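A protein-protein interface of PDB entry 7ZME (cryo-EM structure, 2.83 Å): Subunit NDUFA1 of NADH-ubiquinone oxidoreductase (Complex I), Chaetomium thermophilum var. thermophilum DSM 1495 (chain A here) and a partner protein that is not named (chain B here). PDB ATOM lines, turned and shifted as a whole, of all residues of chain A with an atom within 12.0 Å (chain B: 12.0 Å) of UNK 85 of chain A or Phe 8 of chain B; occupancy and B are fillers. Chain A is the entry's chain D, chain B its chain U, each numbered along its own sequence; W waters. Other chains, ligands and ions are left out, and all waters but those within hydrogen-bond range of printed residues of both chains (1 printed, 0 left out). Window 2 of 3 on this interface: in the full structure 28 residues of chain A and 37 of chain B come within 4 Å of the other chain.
The backbone NH (N) of Val 81 of chain A is in hydrogen-bond range of the backbone carbonyl oxygen (O) of His 11 of chain B, 2.7 Å away. N of Gln 10 of chain B lies within hydrogen-bond range of O of Val 81 of chain A (3.4 Å). The guanidinium group of Arg 4 of chain B is in hydrogen-bond range of O of UNK 85 of chain A (2.8 Å). The backbone NH of Leu 13 of chain B lies within hydrogen-bond range of the backbone carbonyl oxygen of Trp 79 of chain A.
Among the printed residues, merely in contact across the chains: UNK 85 of chain A with Phe 8 of chain B, Gln 44 of chain A with Lys 5 of chain B, UNK 86 of chain A with Arg 4 of chain B, Trp 79 of chain A with Met 1 of chain B, Trp 79 of chain A with Val 12 of chain B, Val 81 of chain A with Asn 9 of chain B, Val 81 of chain A with Leu 13 of chain B, Lys 80 of chain A with His 11 of chain B, Lys 80 of chain A with Asn 9 of chain B, Trp 79 of chain A with His 11 of chain B, Val 81 of chain A with Val 12 of chain B, Lys 80 of chain A with Pro 6 of chain B and UNK 82 of chain A with Phe 8 of chain B.
No residue of chain B comes within 4 Å of UNK 84 of chain A. UNK 85 of chain A touches just these residues of chain B: Arg 4 (2.8 Å) and Phe 8 (3.3 Å). UNK 86 of chain A touches just one residue of chain B: Arg 4. Of the printed residues of chain A, Met 1 of chain B touches Trp 79. Ala 2 of chain B touches none of the printed residues of chain A. Thr 3 of chain B touches none of the printed residues of chain A. Printed residues of chain A within 4 Å of Arg 4 of chain B: UNK 85 and UNK 86. Of the printed residues of chain A, Lys 5 of chain B touches Gln 44. Pro 6 of chain B touches just one residue of chain A: Lys 80 (3.9 Å). No residue of chain A comes within 4 Å of Ala 7 of chain B. Printed residues of chain A within 4 Å of Phe 8 of chain B: UNK 82 (3.98 Å) and UNK 85 (3.3 Å). Of chain A, only Lys 80 (3.7 Å) and Val 81 (3.5 Å) come within 4 Å of Asn 9 of chain B. Gln 10 of chain B touches just one residue of chain A: Val 81. Of the printed residues of chain A, His 11 of chain B touches Trp 79, Lys 80 and Val 81. Of the printed residues of chain A, Val 12 of chain B touches Trp 79 and Val 81. The nearest residue of chain B that does not touch UNK 85 of chain A is Ala 7 of chain B (4.1 Å). The nearest printed residue of chain A that does not touch Lys 5 of chain B is UNK 85 of chain A (5.4 Å).
Of the 10 printed residues of chain A, 7 touch a printed residue of chain B. Hydrophobic or aromatic side chains of chain A that line the printed part of chain B: Trp 79 and Val 81.
Water W1 lies within hydrogen-bond range of O of Lys 5 of chain B (3.1 Å), O of UNK 85 of chain A (3.1 Å) and NH2 of Arg 4 of chain B (3.1 Å).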
ATOM      1  N   GLN A  44     -19.680  30.697 -13.115  1.00  0.00           N
ATOM      2  CA  GLN A  44     -19.351  29.327 -12.661  1.00  0.00           C
ATOM      3  C   GLN A  44     -18.391  29.360 -11.471  1.00  0.00           C
ATOM      4  O   GLN A  44     -18.592  28.560 -10.556  1.00  0.00           O
ATOM      5  CB  GLN A  44     -18.861  28.477 -13.834  1.00  0.00           C
ATOM      6  CG  GLN A  44     -18.619  27.011 -13.494  1.00  0.00           C
ATOM      7  CD  GLN A  44     -19.789  26.280 -12.875  1.00  0.00           C
ATOM      8  OE1 GLN A  44     -19.617  25.288 -12.174  1.00  0.00           O
ATOM      9  NE2 GLN A  44     -21.000  26.749 -13.132  1.00  0.00           N
ATOM     10  N   GLU A  51     -20.445  26.785  -3.262  1.00  0.00           N
ATOM     11  CA  GLU A  51     -20.717  25.361  -2.967  1.00  0.00           C
ATOM     12  C   GLU A  51     -19.551  24.853  -2.128  1.00  0.00           C
ATOM     13  O   GLU A  51     -19.782  23.968  -1.294  1.00  0.00           O
ATOM     14  CB  GLU A  51     -20.836  24.590  -4.275  1.00  0.00           C
ATOM     15  CG  GLU A  51     -22.209  24.683  -4.906  1.00  0.00           C
ATOM     16  CD  GLU A  51     -22.234  24.276  -6.368  1.00  0.00           C
ATOM     17  OE1 GLU A  51     -21.148  24.215  -6.977  1.00  0.00           O
ATOM     18  OE2 GLU A  51     -23.338  24.022  -6.891  1.00  0.00           O
ATOM     19  N   TRP A  79     -20.915  15.670  -6.094  1.00  0.00           N
ATOM     20  CA  TRP A  79     -20.934  15.389  -7.520  1.00  0.00           C
ATOM     21  C   TRP A  79     -22.387  15.383  -7.969  1.00  0.00           C
ATOM     22  O   TRP A  79     -23.182  14.569  -7.496  1.00  0.00           O
ATOM     23  CB  TRP A  79     -20.241  14.064  -7.829  1.00  0.00           C
ATOM     24  CG  TRP A  79     -18.762  14.213  -7.966  1.00  0.00           C
ATOM     25  CD1 TRP A  79     -18.008  15.249  -7.519  1.00  0.00           C
ATOM     26  CD2 TRP A  79     -17.858  13.302  -8.597  1.00  0.00           C
ATOM     27  NE1 TRP A  79     -16.690  15.045  -7.826  1.00  0.00           N
ATOM     28  CE2 TRP A  79     -16.570  13.853  -8.488  1.00  0.00           C
ATOM     29  CE3 TRP A  79     -18.015  12.070  -9.243  1.00  0.00           C
ATOM     30  CZ2 TRP A  79     -15.444  13.221  -9.000  1.00  0.00           C
ATOM     31  CZ3 TRP A  79     -16.894  11.444  -9.749  1.00  0.00           C
ATOM     32  CH2 TRP A  79     -15.626  12.021  -9.626  1.00  0.00           C
ATOM     33  N   LYS A  80     -22.727  16.299  -8.871  1.00  0.00           N
ATOM     34  CA  LYS A  80     -24.118  16.499  -9.245  1.00  0.00           C
ATOM     35  C   LYS A  80     -24.627  15.309 -10.045  1.00  0.00           C
ATOM     36  O   LYS A  80     -23.953  14.811 -10.948  1.00  0.00           O
ATOM     37  CB  LYS A  80     -24.270  17.776 -10.066  1.00  0.00           C
ATOM     38  CG  LYS A  80     -23.777  19.033  -9.387  1.00  0.00           C
ATOM     39  CD  LYS A  80     -24.458  19.282  -8.074  1.00  0.00           C
ATOM     40  CE  LYS A  80     -23.793  20.437  -7.357  1.00  0.00           C
ATOM     41  NZ  LYS A  80     -22.985  19.979  -6.202  1.00  0.00           N
ATOM     42  N   VAL A  81     -25.834  14.862  -9.720  1.00  0.00           N
ATOM     43  CA  VAL A  81     -26.436  13.693 -10.346  1.00  0.00           C
ATOM     44  C   VAL A  81     -27.684  14.148 -11.086  1.00  0.00           C
ATOM     45  O   VAL A  81     -28.588  14.740 -10.486  1.00  0.00           O
ATOM     46  CB  VAL A  81     -26.774  12.609  -9.312  1.00  0.00           C
ATOM     47  CG1 VAL A  81     -27.246  11.362 -10.002  1.00  0.00           C
ATOM     48  CG2 VAL A  81     -25.572  12.314  -8.446  1.00  0.00           C
ATOM     49  N   UNK A  82     -27.729  13.880 -12.386  1.00  0.00           N
ATOM     50  CA  UNK A  82     -28.862  14.230 -13.225  1.00  0.00           C
ATOM     51  C   UNK A  82     -29.347  12.998 -13.973  1.00  0.00           C
ATOM     52  O   UNK A  82     -28.672  11.970 -14.032  1.00  0.00           O
ATOM     53  CB  UNK A  82     -28.508  15.344 -14.220  1.00  0.00           C
ATOM     54  N   UNK A  83     -30.542  13.113 -14.546  1.00  0.00           N
ATOM     55  CA  UNK A  83     -31.118  12.021 -15.317  1.00  0.00           C
ATOM     56  C   UNK A  83     -31.049  12.228 -16.821  1.00  0.00           C
ATOM     57  O   UNK A  83     -30.845  11.251 -17.550  1.00  0.00           O
ATOM     58  CB  UNK A  83     -32.579  11.797 -14.912  1.00  0.00           C
ATOM     59  N   UNK A  84     -31.139  13.478 -17.307  1.00  0.00           N
ATOM     60  CA  UNK A  84     -31.222  13.632 -18.781  1.00  0.00           C
ATOM     61  C   UNK A  84     -30.313  14.676 -19.432  1.00  0.00           C
ATOM     62  O   UNK A  84     -29.855  14.391 -20.555  1.00  0.00           O
ATOM     63  CB  UNK A  84     -32.663  13.860 -19.192  1.00  0.00           C
ATOM     64  N   UNK A  85     -30.024  15.807 -18.790  1.00  0.00           N
ATOM     65  CA  UNK A  85     -29.332  16.908 -19.510  1.00  0.00           C
ATOM     66  C   UNK A  85     -27.816  16.795 -19.613  1.00  0.00           C
ATOM     67  O   UNK A  85     -27.150  17.665 -19.044  1.00  0.00           O
ATOM     68  CB  UNK A  85     -29.673  18.210 -18.875  1.00  0.00           C
ATOM     69  N   UNK A  86     -27.307  15.813 -20.349  1.00  0.00           N
ATOM     70  CA  UNK A  86     -25.864  15.768 -20.627  1.00  0.00           C
ATOM     71  C   UNK A  86     -25.654  16.291 -22.049  1.00  0.00           C
ATOM     72  O   UNK A  86     -26.212  17.372 -22.330  1.00  0.00           O
ATOM     73  CB  UNK A  86     -25.362  14.363 -20.483  1.00  0.00           C
ATOM     74  N   MET B   1     -15.981  13.624 -12.604  1.00  0.00           N
ATOM     75  CA  MET B   1     -17.237  13.783 -13.317  1.00  0.00           C
ATOM     76  C   MET B   1     -17.159  14.970 -14.269  1.00  0.00           C
ATOM     77  O   MET B   1     -16.299  15.832 -14.119  1.00  0.00           O
ATOM     78  CB  MET B   1     -18.380  13.942 -12.324  1.00  0.00           C
ATOM     79  N   ALA B   2     -17.964  14.940 -15.335  1.00  0.00           N
ATOM     80  CA  ALA B   2     -18.037  16.031 -16.339  1.00  0.00           C
ATOM     81  C   ALA B   2     -17.989  17.483 -15.873  1.00  0.00           C
ATOM     82  O   ALA B   2     -18.508  17.807 -14.802  1.00  0.00           O
ATOM     83  CB  ALA B   2     -19.210  15.788 -17.238  1.00  0.00           C
ATOM     84  N   THR B   3     -17.398  18.330 -16.721  1.00  0.00           N
ATOM     85  CA  THR B   3     -17.226  19.764 -16.393  1.00  0.00           C
ATOM     86  C   THR B   3     -18.426  20.550 -16.925  1.00  0.00           C
ATOM     87  O   THR B   3     -18.421  21.786 -16.800  1.00  0.00           O
ATOM     88  CB  THR B   3     -15.907  20.261 -16.983  1.00  0.00           C
ATOM     89  OG1 THR B   3     -16.102  20.402 -18.390  1.00  0.00           O
ATOM     90  CG2 THR B   3     -14.756  19.318 -16.724  1.00  0.00           C
ATOM     91  N   ARG B   4     -19.406  19.850 -17.494  1.00  0.00           N
ATOM     92  CA  ARG B   4     -20.626  20.516 -17.993  1.00  0.00           C
ATOM     93  C   ARG B   4     -21.432  21.018 -16.801  1.00  0.00           C
ATOM     94  O   ARG B   4     -21.473  20.320 -15.777  1.00  0.00           O
ATOM     95  CB  ARG B   4     -21.434  19.591 -18.904  1.00  0.00           C
ATOM     96  CG  ARG B   4     -21.887  18.287 -18.268  1.00  0.00           C
ATOM     97  CD  ARG B   4     -23.070  17.735 -19.035  1.00  0.00           C
ATOM     98  NE  ARG B   4     -23.760  16.701 -18.284  1.00  0.00           N
ATOM     99  CZ  ARG B   4     -24.744  16.927 -17.423  1.00  0.00           C
ATOM    100  NH1 ARG B   4     -25.317  15.919 -16.791  1.00  0.00           N
ATOM    101  NH2 ARG B   4     -25.153  18.162 -17.194  1.00  0.00           N
ATOM    102  N   LYS B   5     -22.041  22.197 -16.943  1.00  0.00           N
ATOM    103  CA  LYS B   5     -22.879  22.748 -15.856  1.00  0.00           C
ATOM    104  C   LYS B   5     -24.244  22.058 -15.907  1.00  0.00           C
ATOM    105  O   LYS B   5     -24.902  22.128 -16.955  1.00  0.00           O
ATOM    106  CB  LYS B   5     -22.996  24.260 -16.024  1.00  0.00           C
ATOM    107  CG  LYS B   5     -21.670  25.004 -16.131  1.00  0.00           C
ATOM    108  CD  LYS B   5     -21.840  26.502 -16.275  1.00  0.00           C
ATOM    109  CE  LYS B   5     -22.678  26.892 -17.474  1.00  0.00           C
ATOM    110  NZ  LYS B   5     -22.044  26.467 -18.744  1.00  0.00           N
ATOM    111  N   PRO B   6     -24.691  21.401 -14.814  1.00  0.00           N
ATOM    112  CA  PRO B   6     -25.957  20.670 -14.810  1.00  0.00           C
ATOM    113  C   PRO B   6     -27.206  21.544 -14.986  1.00  0.00           C
ATOM    114  O   PRO B   6     -27.223  22.644 -14.471  1.00  0.00           O
ATOM    115  CB  PRO B   6     -25.964  20.041 -13.410  1.00  0.00           C
ATOM    116  CG  PRO B   6     -25.077  20.930 -12.580  1.00  0.00           C
ATOM    117  CD  PRO B   6     -23.981  21.326 -13.538  1.00  0.00           C
ATOM    118  N   ALA B   7     -28.216  21.043 -15.698  1.00  0.00           N
ATOM    119  CA  ALA B   7     -29.458  21.783 -15.841  1.00  0.00           C
ATOM    120  C   ALA B   7     -30.629  21.139 -15.125  1.00  0.00           C
ATOM    121  O   ALA B   7     -31.648  21.801 -14.926  1.00  0.00           O
ATOM    122  CB  ALA B   7     -29.817  21.950 -17.326  1.00  0.00           C
ATOM    123  N   PHE B   8     -30.511  19.872 -14.732  1.00  0.00           N
ATOM    124  CA  PHE B   8     -31.593  19.143 -14.083  1.00  0.00           C
ATOM    125  C   PHE B   8     -31.095  18.317 -12.904  1.00  0.00           C
ATOM    126  O   PHE B   8     -31.628  17.237 -12.637  1.00  0.00           O
ATOM    127  CB  PHE B   8     -32.314  18.253 -15.097  1.00  0.00           C
ATOM    128  CG  PHE B   8     -33.007  19.019 -16.183  1.00  0.00           C
ATOM    129  CD1 PHE B   8     -34.249  19.576 -15.974  1.00  0.00           C
ATOM    130  CD2 PHE B   8     -32.405  19.196 -17.412  1.00  0.00           C
ATOM    131  CE1 PHE B   8     -34.878  20.282 -16.970  1.00  0.00           C
ATOM    132  CE2 PHE B   8     -33.028  19.903 -18.410  1.00  0.00           C
ATOM    133  CZ  PHE B   8     -34.270  20.446 -18.189  1.00  0.00           C
ATOM    134  N   ASN B   9     -30.076  18.796 -12.201  1.00  0.00           N
ATOM    135  CA  ASN B   9     -29.537  18.066 -11.063  1.00  0.00           C
ATOM    136  C   ASN B   9     -30.486  18.173  -9.875  1.00  0.00           C
ATOM    137  O   ASN B   9     -30.923  19.268  -9.513  1.00  0.00           O
ATOM    138  CB  ASN B   9     -28.160  18.608 -10.694  1.00  0.00           C
ATOM    139  CG  ASN B   9     -28.155  20.111 -10.520  1.00  0.00           C
ATOM    140  OD1 ASN B   9     -28.587  20.849 -11.402  1.00  0.00           O
ATOM    141  ND2 ASN B   9     -27.665  20.573  -9.381  1.00  0.00           N
ATOM    142  N   GLN B  10     -30.807  17.033  -9.274  1.00  0.00           N
ATOM    143  CA  GLN B  10     -31.583  16.988  -8.047  1.00  0.00           C
ATOM    144  C   GLN B  10     -30.909  16.148  -6.976  1.00  0.00           C
ATOM    145  O   GLN B  10     -31.477  15.986  -5.892  1.00  0.00           O
ATOM    146  CB  GLN B  10     -32.990  16.432  -8.311  1.00  0.00           C
ATOM    147  CG  GLN B  10     -33.730  17.108  -9.446  1.00  0.00           C
ATOM    148  CD  GLN B  10     -34.449  18.361  -8.999  1.00  0.00           C
ATOM    149  OE1 GLN B  10     -34.157  19.458  -9.469  1.00  0.00           O
ATOM    150  NE2 GLN B  10     -35.397  18.204  -8.082  1.00  0.00           N
ATOM    151  N   HIS B  11     -29.725  15.621  -7.266  1.00  0.00           N
ATOM    152  CA  HIS B  11     -29.083  14.672  -6.327  1.00  0.00           C
ATOM    153  C   HIS B  11     -27.580  14.842  -6.310  1.00  0.00           C
ATOM    154  O   HIS B  11     -27.025  15.290  -7.310  1.00  0.00           O
ATOM    155  CB  HIS B  11     -29.389  13.224  -6.733  1.00  0.00           C
ATOM    156  CG  HIS B  11     -30.818  12.839  -6.567  1.00  0.00           C
ATOM    157  ND1 HIS B  11     -31.378  12.617  -5.329  1.00  0.00           N
ATOM    158  CD2 HIS B  11     -31.798  12.645  -7.472  1.00  0.00           C
ATOM    159  CE1 HIS B  11     -32.647  12.302  -5.474  1.00  0.00           C
ATOM    160  NE2 HIS B  11     -32.929  12.312  -6.781  1.00  0.00           N
ATOM    161  N   VAL B  12     -26.985  14.585  -5.152  1.00  0.00           N
ATOM    162  CA  VAL B  12     -25.509  14.659  -5.009  1.00  0.00           C
ATOM    163  C   VAL B  12     -25.004  13.249  -4.684  1.00  0.00           C
ATOM    164  O   VAL B  12     -25.647  12.574  -3.870  1.00  0.00           O
ATOM    165  CB  VAL B  12     -25.146  15.680  -3.915  1.00  0.00           C
ATOM    166  CG1 VAL B  12     -23.793  15.403  -3.288  1.00  0.00           C
ATOM    167  CG2 VAL B  12     -25.239  17.111  -4.421  1.00  0.00           C
ATOM    168  N   LEU B  13     -23.936  12.799  -5.343  1.00  0.00           N
ATOM    169  CA  LEU B  13     -23.325  11.483  -5.025  1.00  0.00           C
ATOM    170  C   LEU B  13     -22.020  11.751  -4.277  1.00  0.00           C
ATOM    171  O   LEU B  13     -21.258  12.608  -4.735  1.00  0.00           O
ATOM    172  CB  LEU B  13     -23.080  10.708  -6.321  1.00  0.00           C
ATOM    173  CG  LEU B  13     -22.736   9.230  -6.162  1.00  0.00           C
ATOM    174  CD1 LEU B  13     -23.845   8.486  -5.434  1.00  0.00           C
ATOM    175  CD2 LEU B  13     -22.480   8.603  -7.520  1.00  0.00           C
HETATM  176  O   HOH W   1     -25.609  20.341 -19.360  1.00  0.00           O
